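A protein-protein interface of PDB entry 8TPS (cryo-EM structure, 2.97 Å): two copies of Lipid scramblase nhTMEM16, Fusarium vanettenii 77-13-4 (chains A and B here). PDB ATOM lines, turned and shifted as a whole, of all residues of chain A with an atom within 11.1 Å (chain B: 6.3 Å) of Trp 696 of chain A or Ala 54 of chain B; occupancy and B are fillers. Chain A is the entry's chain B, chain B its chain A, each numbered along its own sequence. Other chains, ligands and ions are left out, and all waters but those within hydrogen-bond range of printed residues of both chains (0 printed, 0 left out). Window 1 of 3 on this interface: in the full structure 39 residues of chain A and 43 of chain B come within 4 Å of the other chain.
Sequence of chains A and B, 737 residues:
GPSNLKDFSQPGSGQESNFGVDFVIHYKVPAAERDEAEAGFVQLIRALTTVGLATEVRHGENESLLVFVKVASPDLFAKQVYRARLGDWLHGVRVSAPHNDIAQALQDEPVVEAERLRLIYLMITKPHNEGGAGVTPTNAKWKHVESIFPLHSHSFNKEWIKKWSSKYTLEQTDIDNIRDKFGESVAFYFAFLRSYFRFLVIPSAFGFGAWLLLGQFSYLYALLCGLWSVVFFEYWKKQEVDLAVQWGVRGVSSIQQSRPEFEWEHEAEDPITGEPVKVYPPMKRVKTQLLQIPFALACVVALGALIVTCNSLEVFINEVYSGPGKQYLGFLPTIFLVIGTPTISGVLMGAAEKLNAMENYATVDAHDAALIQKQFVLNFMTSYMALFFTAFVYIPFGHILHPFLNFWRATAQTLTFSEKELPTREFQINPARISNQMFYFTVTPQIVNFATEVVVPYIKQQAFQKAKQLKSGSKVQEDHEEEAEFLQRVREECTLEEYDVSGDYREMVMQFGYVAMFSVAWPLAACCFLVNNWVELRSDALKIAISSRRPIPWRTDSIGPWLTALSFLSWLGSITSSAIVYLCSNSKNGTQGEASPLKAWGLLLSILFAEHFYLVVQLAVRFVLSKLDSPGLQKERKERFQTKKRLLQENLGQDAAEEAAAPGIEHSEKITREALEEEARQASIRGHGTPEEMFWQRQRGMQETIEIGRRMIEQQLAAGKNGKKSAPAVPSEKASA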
ATOM      1  N   PRO A 691      21.986  20.763  20.499  1.00  0.00           N
ATOM      2  CA  PRO A 691      22.458  21.904  19.706  1.00  0.00           C
ATOM      3  C   PRO A 691      21.312  22.784  19.214  1.00  0.00           C
ATOM      4  O   PRO A 691      20.300  22.916  19.900  1.00  0.00           O
ATOM      5  CB  PRO A 691      23.181  21.243  18.526  1.00  0.00           C
ATOM      6  CG  PRO A 691      22.627  19.861  18.457  1.00  0.00           C
ATOM      7  CD  PRO A 691      22.312  19.474  19.865  1.00  0.00           C
ATOM      8  N   GLU A 692      21.485  23.382  18.033  1.00  0.00           N
ATOM      9  CA  GLU A 692      20.447  24.237  17.469  1.00  0.00           C
ATOM     10  C   GLU A 692      19.181  23.449  17.146  1.00  0.00           C
ATOM     11  O   GLU A 692      18.069  23.935  17.384  1.00  0.00           O
ATOM     12  CB  GLU A 692      20.970  24.941  16.217  1.00  0.00           C
ATOM     13  N   GLU A 693      19.330  22.241  16.597  1.00  0.00           N
ATOM     14  CA  GLU A 693      18.163  21.432  16.258  1.00  0.00           C
ATOM     15  C   GLU A 693      17.355  21.058  17.493  1.00  0.00           C
ATOM     16  O   GLU A 693      16.123  21.149  17.474  1.00  0.00           O
ATOM     17  CB  GLU A 693      18.598  20.173  15.507  1.00  0.00           C
ATOM     18  N   MET A 694      18.023  20.642  18.573  1.00  0.00           N
ATOM     19  CA  MET A 694      17.307  20.330  19.803  1.00  0.00           C
ATOM     20  C   MET A 694      16.698  21.579  20.427  1.00  0.00           C
ATOM     21  O   MET A 694      15.625  21.508  21.036  1.00  0.00           O
ATOM     22  CB  MET A 694      18.243  19.642  20.797  1.00  0.00           C
ATOM     23  N   PHE A 695      17.368  22.724  20.288  1.00  0.00           N
ATOM     24  CA  PHE A 695      16.840  23.969  20.834  1.00  0.00           C
ATOM     25  C   PHE A 695      15.593  24.423  20.085  1.00  0.00           C
ATOM     26  O   PHE A 695      14.682  25.010  20.680  1.00  0.00           O
ATOM     27  CB  PHE A 695      17.919  25.053  20.792  1.00  0.00           C
ATOM     28  CG  PHE A 695      17.386  26.452  20.916  1.00  0.00           C
ATOM     29  CD1 PHE A 695      16.988  26.953  22.143  1.00  0.00           C
ATOM     30  CD2 PHE A 695      17.294  27.272  19.802  1.00  0.00           C
ATOM     31  CE1 PHE A 695      16.500  28.241  22.257  1.00  0.00           C
ATOM     32  CE2 PHE A 695      16.808  28.560  19.909  1.00  0.00           C
ATOM     33  CZ  PHE A 695      16.410  29.045  21.138  1.00  0.00           C
ATOM     34  N   TRP A 696      15.533  24.165  18.780  1.00  0.00           N
ATOM     35  CA  TRP A 696      14.443  24.666  17.955  1.00  0.00           C
ATOM     36  C   TRP A 696      13.298  23.677  17.786  1.00  0.00           C
ATOM     37  O   TRP A 696      12.272  24.039  17.199  1.00  0.00           O
ATOM     38  CB  TRP A 696      14.974  25.069  16.576  1.00  0.00           C
ATOM     39  CG  TRP A 696      15.531  26.455  16.548  1.00  0.00           C
ATOM     40  CD1 TRP A 696      16.837  26.810  16.375  1.00  0.00           C
ATOM     41  CD2 TRP A 696      14.803  27.675  16.722  1.00  0.00           C
ATOM     42  NE1 TRP A 696      16.964  28.177  16.416  1.00  0.00           N
ATOM     43  CE2 TRP A 696      15.729  28.731  16.627  1.00  0.00           C
ATOM     44  CE3 TRP A 696      13.455  27.978  16.934  1.00  0.00           C
ATOM     45  CZ2 TRP A 696      15.352  30.066  16.743  1.00  0.00           C
ATOM     46  CZ3 TRP A 696      13.083  29.304  17.050  1.00  0.00           C
ATOM     47  CH2 TRP A 696      14.027  30.331  16.954  1.00  0.00           C
ATOM     48  N   GLN A 697      13.436  22.445  18.278  1.00  0.00           N
ATOM     49  CA  GLN A 697      12.376  21.451  18.196  1.00  0.00           C
ATOM     50  C   GLN A 697      11.605  21.298  19.502  1.00  0.00           C
ATOM     51  O   GLN A 697      10.928  20.281  19.694  1.00  0.00           O
ATOM     52  CB  GLN A 697      12.949  20.101  17.758  1.00  0.00           C
ATOM     53  CG  GLN A 697      12.609  19.720  16.324  1.00  0.00           C
ATOM     54  CD  GLN A 697      13.513  20.385  15.303  1.00  0.00           C
ATOM     55  OE1 GLN A 697      14.721  20.157  15.284  1.00  0.00           O
ATOM     56  NE2 GLN A 697      12.928  21.214  14.447  1.00  0.00           N
ATOM     57  N   ARG A 698      11.691  22.279  20.400  1.00  0.00           N
ATOM     58  CA  ARG A 698      10.947  22.212  21.652  1.00  0.00           C
ATOM     59  C   ARG A 698       9.471  22.527  21.428  1.00  0.00           C
ATOM     60  O   ARG A 698       8.596  21.710  21.730  1.00  0.00           O
ATOM     61  CB  ARG A 698      11.560  23.170  22.676  1.00  0.00           C
ATOM     62  CG  ARG A 698      13.075  23.091  22.757  1.00  0.00           C
ATOM     63  CD  ARG A 698      13.534  22.271  23.951  1.00  0.00           C
ATOM     64  NE  ARG A 698      14.843  22.700  24.428  1.00  0.00           N
ATOM     65  CZ  ARG A 698      15.422  22.250  25.533  1.00  0.00           C
ATOM     66  NH1 ARG A 698      14.835  21.349  26.304  1.00  0.00           N
ATOM     67  NH2 ARG A 698      16.620  22.715  25.873  1.00  0.00           N
ATOM     68  N   GLN A 699       9.181  23.713  20.896  1.00  0.00           N
ATOM     69  CA  GLN A 699       7.825  24.126  20.533  1.00  0.00           C
ATOM     70  C   GLN A 699       7.815  24.358  19.025  1.00  0.00           C
ATOM     71  O   GLN A 699       8.034  25.473  18.549  1.00  0.00           O
ATOM     72  CB  GLN A 699       7.406  25.377  21.307  1.00  0.00           C
ATOM     73  CG  GLN A 699       7.900  25.405  22.743  1.00  0.00           C
ATOM     74  CD  GLN A 699       8.319  26.793  23.187  1.00  0.00           C
ATOM     75  OE1 GLN A 699       8.053  27.783  22.504  1.00  0.00           O
ATOM     76  NE2 GLN A 699       8.982  26.872  24.335  1.00  0.00           N
ATOM     77  N   ARG A 700       7.557  23.288  18.273  1.00  0.00           N
ATOM     78  CA  ARG A 700       7.639  23.328  16.819  1.00  0.00           C
ATOM     79  C   ARG A 700       6.451  24.023  16.169  1.00  0.00           C
ATOM     80  O   ARG A 700       6.548  24.407  14.998  1.00  0.00           O
ATOM     81  CB  ARG A 700       7.768  21.906  16.269  1.00  0.00           C
ATOM     82  CG  ARG A 700       6.663  20.966  16.722  1.00  0.00           C
ATOM     83  CD  ARG A 700       7.053  19.510  16.518  1.00  0.00           C
ATOM     84  NE  ARG A 700       8.213  19.140  17.319  1.00  0.00           N
ATOM     85  CZ  ARG A 700       8.161  18.781  18.594  1.00  0.00           C
ATOM     86  NH1 ARG A 700       7.014  18.728  19.252  1.00  0.00           N
ATOM     87  NH2 ARG A 700       9.287  18.463  19.226  1.00  0.00           N
ATOM     88  N   GLY A 701       5.343  24.197  16.891  1.00  0.00           N
ATOM     89  CA  GLY A 701       4.155  24.817  16.352  1.00  0.00           C
ATOM     90  C   GLY A 701       3.793  26.115  17.057  1.00  0.00           C
ATOM     91  O   GLY A 701       4.613  26.758  17.715  1.00  0.00           O
ATOM     92  N   MET A 702       2.525  26.501  16.902  1.00  0.00           N
ATOM     93  CA  MET A 702       1.986  27.728  17.477  1.00  0.00           C
ATOM     94  C   MET A 702       1.183  27.483  18.749  1.00  0.00           C
ATOM     95  O   MET A 702       1.304  28.249  19.711  1.00  0.00           O
ATOM     96  CB  MET A 702       1.109  28.450  16.445  1.00  0.00           C
ATOM     97  CG  MET A 702       0.422  29.705  16.965  1.00  0.00           C
ATOM     98  SD  MET A 702      -1.202  29.990  16.232  1.00  0.00           S
ATOM     99  CE  MET A 702      -0.753  30.582  14.603  1.00  0.00           C
ATOM    100  N   GLU A 704       1.467  25.031  21.056  1.00  0.00           N
ATOM    101  CA  GLU A 704       2.379  24.820  22.172  1.00  0.00           C
ATOM    102  C   GLU A 704       3.099  26.113  22.532  1.00  0.00           C
ATOM    103  O   GLU A 704       3.422  26.336  23.701  1.00  0.00           O
ATOM    104  CB  GLU A 704       3.394  23.718  21.843  1.00  0.00           C
ATOM    105  CG  GLU A 704       4.060  23.806  20.468  1.00  0.00           C
ATOM    106  CD  GLU A 704       3.157  23.410  19.307  1.00  0.00           C
ATOM    107  OE1 GLU A 704       3.493  22.432  18.609  1.00  0.00           O
ATOM    108  OE2 GLU A 704       2.127  24.075  19.081  1.00  0.00           O
ATOM    109  N   THR A 705       3.345  26.980  21.544  1.00  0.00           N
ATOM    110  CA  THR A 705       4.080  28.215  21.808  1.00  0.00           C
ATOM    111  C   THR A 705       3.326  29.121  22.775  1.00  0.00           C
ATOM    112  O   THR A 705       3.883  29.542  23.794  1.00  0.00           O
ATOM    113  CB  THR A 705       4.376  28.941  20.494  1.00  0.00           C
ATOM    114  OG1 THR A 705       5.269  28.147  19.701  1.00  0.00           O
ATOM    115  CG2 THR A 705       5.024  30.297  20.755  1.00  0.00           C
ATOM    116  N   ILE A 708       2.911  27.421  26.291  1.00  0.00           N
ATOM    117  CA  ILE A 708       4.092  27.536  27.132  1.00  0.00           C
ATOM    118  C   ILE A 708       4.306  28.986  27.536  1.00  0.00           C
ATOM    119  O   ILE A 708       4.811  29.264  28.622  1.00  0.00           O
ATOM    120  CB  ILE A 708       5.331  26.941  26.435  1.00  0.00           C
ATOM    121  CG1 ILE A 708       6.433  26.665  27.457  1.00  0.00           C
ATOM    122  CG2 ILE A 708       5.864  27.866  25.363  1.00  0.00           C
ATOM    123  CD1 ILE A 708       7.104  25.324  27.273  1.00  0.00           C
ATOM    124  N   PHE B  19      22.441  29.909  17.676  1.00  0.00           N
ATOM    125  CA  PHE B  19      21.671  28.702  17.383  1.00  0.00           C
ATOM    126  C   PHE B  19      20.777  28.886  16.166  1.00  0.00           C
ATOM    127  O   PHE B  19      19.687  28.312  16.091  1.00  0.00           O
ATOM    128  CB  PHE B  19      20.842  28.298  18.597  1.00  0.00           C
ATOM    129  CG  PHE B  19      21.648  27.694  19.709  1.00  0.00           C
ATOM    130  CD1 PHE B  19      22.533  26.659  19.457  1.00  0.00           C
ATOM    131  CD2 PHE B  19      21.521  28.161  21.006  1.00  0.00           C
ATOM    132  CE1 PHE B  19      23.276  26.101  20.481  1.00  0.00           C
ATOM    133  CE2 PHE B  19      22.261  27.608  22.032  1.00  0.00           C
ATOM    134  CZ  PHE B  19      23.140  26.577  21.769  1.00  0.00           C
ATOM    135  N   GLY B  20      21.216  29.683  15.195  1.00  0.00           N
ATOM    136  CA  GLY B  20      20.380  30.010  14.061  1.00  0.00           C
ATOM    137  C   GLY B  20      19.361  31.091  14.321  1.00  0.00           C
ATOM    138  O   GLY B  20      18.525  31.356  13.451  1.00  0.00           O
ATOM    139  N   VAL B  21      19.401  31.720  15.495  1.00  0.00           N
ATOM    140  CA  VAL B  21      18.454  32.777  15.830  1.00  0.00           C
ATOM    141  C   VAL B  21      18.736  33.978  14.937  1.00  0.00           C
ATOM    142  O   VAL B  21      19.886  34.413  14.803  1.00  0.00           O
ATOM    143  CB  VAL B  21      18.555  33.149  17.314  1.00  0.00           C
ATOM    144  CG1 VAL B  21      18.143  34.600  17.538  1.00  0.00           C
ATOM    145  CG2 VAL B  21      17.734  32.197  18.160  1.00  0.00           C
ATOM    146  N   ASP B  22      17.689  34.516  14.316  1.00  0.00           N
ATOM    147  CA  ASP B  22      17.860  35.628  13.393  1.00  0.00           C
ATOM    148  C   ASP B  22      17.353  36.955  13.942  1.00  0.00           C
ATOM    149  O   ASP B  22      17.864  38.007  13.545  1.00  0.00           O
ATOM    150  CB  ASP B  22      17.164  35.320  12.063  1.00  0.00           C
ATOM    151  CG  ASP B  22      18.117  34.736  11.037  1.00  0.00           C
ATOM    152  OD1 ASP B  22      19.089  34.066  11.448  1.00  0.00           O
ATOM    153  OD2 ASP B  22      17.905  34.943   9.826  1.00  0.00           O
ATOM    154  N   LEU B  48       3.322  36.806  14.053  1.00  0.00           N
ATOM    155  CA  LEU B  48       4.623  36.330  13.597  1.00  0.00           C
ATOM    156  C   LEU B  48       4.497  35.016  12.837  1.00  0.00           C
ATOM    157  O   LEU B  48       5.216  34.789  11.857  1.00  0.00           O
ATOM    158  CB  LEU B  48       5.562  36.178  14.793  1.00  0.00           C
ATOM    159  CG  LEU B  48       6.218  37.470  15.289  1.00  0.00           C
ATOM    160  CD1 LEU B  48       7.466  37.159  16.089  1.00  0.00           C
ATOM    161  CD2 LEU B  48       6.541  38.400  14.129  1.00  0.00           C
ATOM    162  N   GLY B  52       5.095  33.430   8.618  1.00  0.00           N
ATOM    163  CA  GLY B  52       5.874  32.232   8.372  1.00  0.00           C
ATOM    164  C   GLY B  52       7.234  32.252   9.037  1.00  0.00           C
ATOM    165  O   GLY B  52       8.250  31.955   8.401  1.00  0.00           O
ATOM    166  N   LEU B  53       7.265  32.602  10.321  1.00  0.00           N
ATOM    167  CA  LEU B  53       8.498  32.717  11.085  1.00  0.00           C
ATOM    168  C   LEU B  53       8.471  31.739  12.251  1.00  0.00           C
ATOM    169  O   LEU B  53       7.511  31.720  13.028  1.00  0.00           O
ATOM    170  CB  LEU B  53       8.683  34.147  11.598  1.00  0.00           C
ATOM    171  CG  LEU B  53       9.004  35.201  10.538  1.00  0.00           C
ATOM    172  CD1 LEU B  53       9.034  36.589  11.150  1.00  0.00           C
ATOM    173  CD2 LEU B  53      10.329  34.887   9.867  1.00  0.00           C
ATOM    174  N   ALA B  54       9.522  30.928  12.369  1.00  0.00           N
ATOM    175  CA  ALA B  54       9.651  30.015  13.497  1.00  0.00           C
ATOM    176  C   ALA B  54      10.037  30.796  14.748  1.00  0.00           C
ATOM    177  O   ALA B  54      10.969  31.609  14.716  1.00  0.00           O
ATOM    178  CB  ALA B  54      10.688  28.938  13.191  1.00  0.00           C
ATOM    179  N   THR B  55       9.328  30.544  15.850  1.00  0.00           N
ATOM    180  CA  THR B  55       9.460  31.318  17.078  1.00  0.00           C
ATOM    181  C   THR B  55       9.703  30.408  18.277  1.00  0.00           C
ATOM    182  O   THR B  55       9.238  29.264  18.312  1.00  0.00           O
ATOM    183  CB  THR B  55       8.207  32.167  17.338  1.00  0.00           C
ATOM    184  OG1 THR B  55       7.109  31.310  17.672  1.00  0.00           O
ATOM    185  CG2 THR B  55       7.847  32.994  16.111  1.00  0.00           C
ATOM    186  N   GLU B  56      10.436  30.938  19.254  1.00  0.00           N
ATOM    187  CA  GLU B  56      10.701  30.281  20.528  1.00  0.00           C
ATOM    188  C   GLU B  56      10.622  31.320  21.640  1.00  0.00           C
ATOM    189  O   GLU B  56      10.865  32.506  21.417  1.00  0.00           O
ATOM    190  CB  GLU B  56      12.077  29.600  20.537  1.00  0.00           C
ATOM    191  CG  GLU B  56      12.090  28.206  21.139  1.00  0.00           C
ATOM    192  CD  GLU B  56      11.319  27.203  20.307  1.00  0.00           C
ATOM    193  OE1 GLU B  56      11.573  27.116  19.088  1.00  0.00           O
ATOM    194  OE2 GLU B  56      10.464  26.493  20.871  1.00  0.00           O
ATOM    195  N   ARG B  58      11.760  32.226  25.730  1.00  0.00           N
ATOM    196  CA  ARG B  58      12.654  31.940  26.847  1.00  0.00           C
ATOM    197  C   ARG B  58      12.602  33.072  27.869  1.00  0.00           C
ATOM    198  O   ARG B  58      12.064  34.154  27.612  1.00  0.00           O
ATOM    199  CB  ARG B  58      14.102  31.730  26.379  1.00  0.00           C
ATOM    200  CG  ARG B  58      14.299  30.597  25.387  1.00  0.00           C
ATOM    201  CD  ARG B  58      13.987  29.255  26.026  1.00  0.00           C
ATOM    202  NE  ARG B  58      13.514  28.285  25.048  1.00  0.00           N
ATOM    203  CZ  ARG B  58      14.233  27.266  24.597  1.00  0.00           C
ATOM    204  NH1 ARG B  58      15.463  27.041  25.035  1.00  0.00           N
ATOM    205  NH2 ARG B  58      13.708  26.452  23.687  1.00  0.00           N
ATOM    206  N   PHE B  68      12.657  34.385  20.205  1.00  0.00           N
ATOM    207  CA  PHE B  68      13.680  34.138  19.200  1.00  0.00           C
ATOM    208  C   PHE B  68      12.996  33.722  17.905  1.00  0.00           C
ATOM    209  O   PHE B  68      12.138  32.836  17.914  1.00  0.00           O
ATOM    210  CB  PHE B  68      14.636  33.042  19.672  1.00  0.00           C
ATOM    211  CG  PHE B  68      15.476  33.440  20.851  1.00  0.00           C
ATOM    212  CD1 PHE B  68      16.555  34.291  20.698  1.00  0.00           C
ATOM    213  CD2 PHE B  68      15.180  32.960  22.116  1.00  0.00           C
ATOM    214  CE1 PHE B  68      17.325  34.655  21.784  1.00  0.00           C
ATOM    215  CE2 PHE B  68      15.948  33.321  23.206  1.00  0.00           C
ATOM    216  CZ  PHE B  68      17.022  34.169  23.039  1.00  0.00           C
ATOM    217  N   VAL B  69      13.371  34.358  16.796  1.00  0.00           N
ATOM    218  CA  VAL B  69      12.646  34.209  15.540  1.00  0.00           C
ATOM    219  C   VAL B  69      13.635  33.944  14.413  1.00  0.00           C
ATOM    220  O   VAL B  69      14.637  34.658  14.280  1.00  0.00           O
ATOM    221  CB  VAL B  69      11.799  35.453  15.227  1.00  0.00           C
ATOM    222  CG1 VAL B  69      11.262  35.394  13.808  1.00  0.00           C
ATOM    223  CG2 VAL B  69      10.664  35.582  16.226  1.00  0.00           C
ATOM    224  N   LYS B  70      13.352  32.921  13.605  1.00  0.00           N
ATOM    225  CA  LYS B  70      14.000  32.746  12.309  1.00  0.00           C
ATOM    226  C   LYS B  70      12.917  32.514  11.262  1.00  0.00           C
ATOM    227  O   LYS B  70      11.719  32.619  11.543  1.00  0.00           O
ATOM    228  CB  LYS B  70      14.986  31.571  12.291  1.00  0.00           C
ATOM    229  CG  LYS B  70      14.331  30.202  12.387  1.00  0.00           C
ATOM    230  CD  LYS B  70      15.132  29.224  13.214  1.00  0.00           C
ATOM    231  CE  LYS B  70      14.311  27.978  13.490  1.00  0.00           C
ATOM    232  NZ  LYS B  70      14.381  27.006  12.364  1.00  0.00           N
ATOM    233  N   VAL B  71      13.341  32.181  10.046  1.00  0.00           N
ATOM    234  CA  VAL B  71      12.409  31.768   9.004  1.00  0.00           C
ATOM    235  C   VAL B  71      12.084  30.287   9.161  1.00  0.00           C
ATOM    236  O   VAL B  71      11.349  29.712   8.358  1.00  0.00           O
ATOM    237  CB  VAL B  71      12.966  32.056   7.600  1.00  0.00           C
ATOM    238  CG1 VAL B  71      13.363  33.513   7.477  1.00  0.00           C
ATOM    239  CG2 VAL B  71      14.153  31.150   7.306  1.00  0.00           C
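O of Phe 19 of chain B is in hydrogen-bond range of NE1 of Trp 696 of chain A (2.7 Å). N of Gln 699 of chain A lies within hydrogen-bond range of OE2 of Glu 56 of chain B (3.1 Å). NH2 of Arg 58 of chain B is in hydrogen-bond range of O of Phe 695 of chain A (3.5 Å).
N of Ala 54 of chain B is in hydrogen-bond range of O of Lys 70 of chain B (2.9 Å). The backbone NH of Phe 68 of chain B lies within hydrogen-bond range of the backbone carbonyl oxygen of Glu 56 of chain B, at 2.9 Å. The side-chain hydroxyl (OG1) of Thr 705 of chain A sits at hydrogen-bond distance from the backbone carbonyl oxygen (O) of Gly 701 of chain A.
Among the printed residues, merely in contact across the chains: Glu 692 of chain A with Phe 19 of chain B, Phe 695 of chain A with Phe 19 of chain B, Trp 696 of chain A with Val 21 of chain B, Trp 696 of chain A with Ala 54 of chain B, Trp 696 of chain A with Thr 55 of chain B, Trp 696 of chain A with Glu 56 of chain B, Trp 696 of chain A with Phe 68 of chain B, Trp 696 of chain A with Lys 70 of chain B, Arg 698 of chain A with Glu 56 of chain B, Arg 698 of chain A with Arg 58 of chain B, Gln 699 of chain A with Thr 55 of chain B and Thr 705 of chain A with Thr 55 of chain B.
Trp 696 of chain A touches seven residues of chain B. Ile 708 of chain A touches none of the printed residues of chain B. Val 21 of chain B touches just one residue of chain A: Trp 696. No residue of chain A comes within 4 Å of Gly 52 of chain B. No residue of chain A comes within 4 Å of Leu 53 of chain B. Of chain A, only Trp 696 comes within 4 Å of Ala 54 of chain B. Of the printed residues of chain A, Thr 55 of chain B touches Trp 696 (3.8 Å), Gln 699 (3.98 Å) and Thr 705 (3.9 Å). Of the printed residues of chain A, Glu 56 of chain B touches Trp 696, Arg 698 and Gln 699. Printed residues of chain A within 4 Å of Phe 68 of chain B: Trp 696. No residue of chain A comes within 4 Å of Val 69 of chain B. Lys 70 of chain B touches one residue of chain A. No residue of chain A comes within 4 Å of Val 71 of chain B. The nearest residue of chain A that does not touch Ala 54 of chain B is Arg 700 of chain A (6.4 Å).
Hydrophobic or aromatic side chains of chain A within 4 Å of the printed part of chain B: Phe 695 and Trp 696. Of the 15 printed residues of chain B, 8 touch a printed residue of chain A. Among the printed residues, 15 pairs touch across the chains. Among the printed residues, no Asp or Glu carboxylate lies within 4 Å of a Lys or Arg side-chain nitrogen of the other chain.
No position is printed for both chains. Of the 15 pairs that touch across the chains among the printed residues, none has its exchanged pair printed and touching as well.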
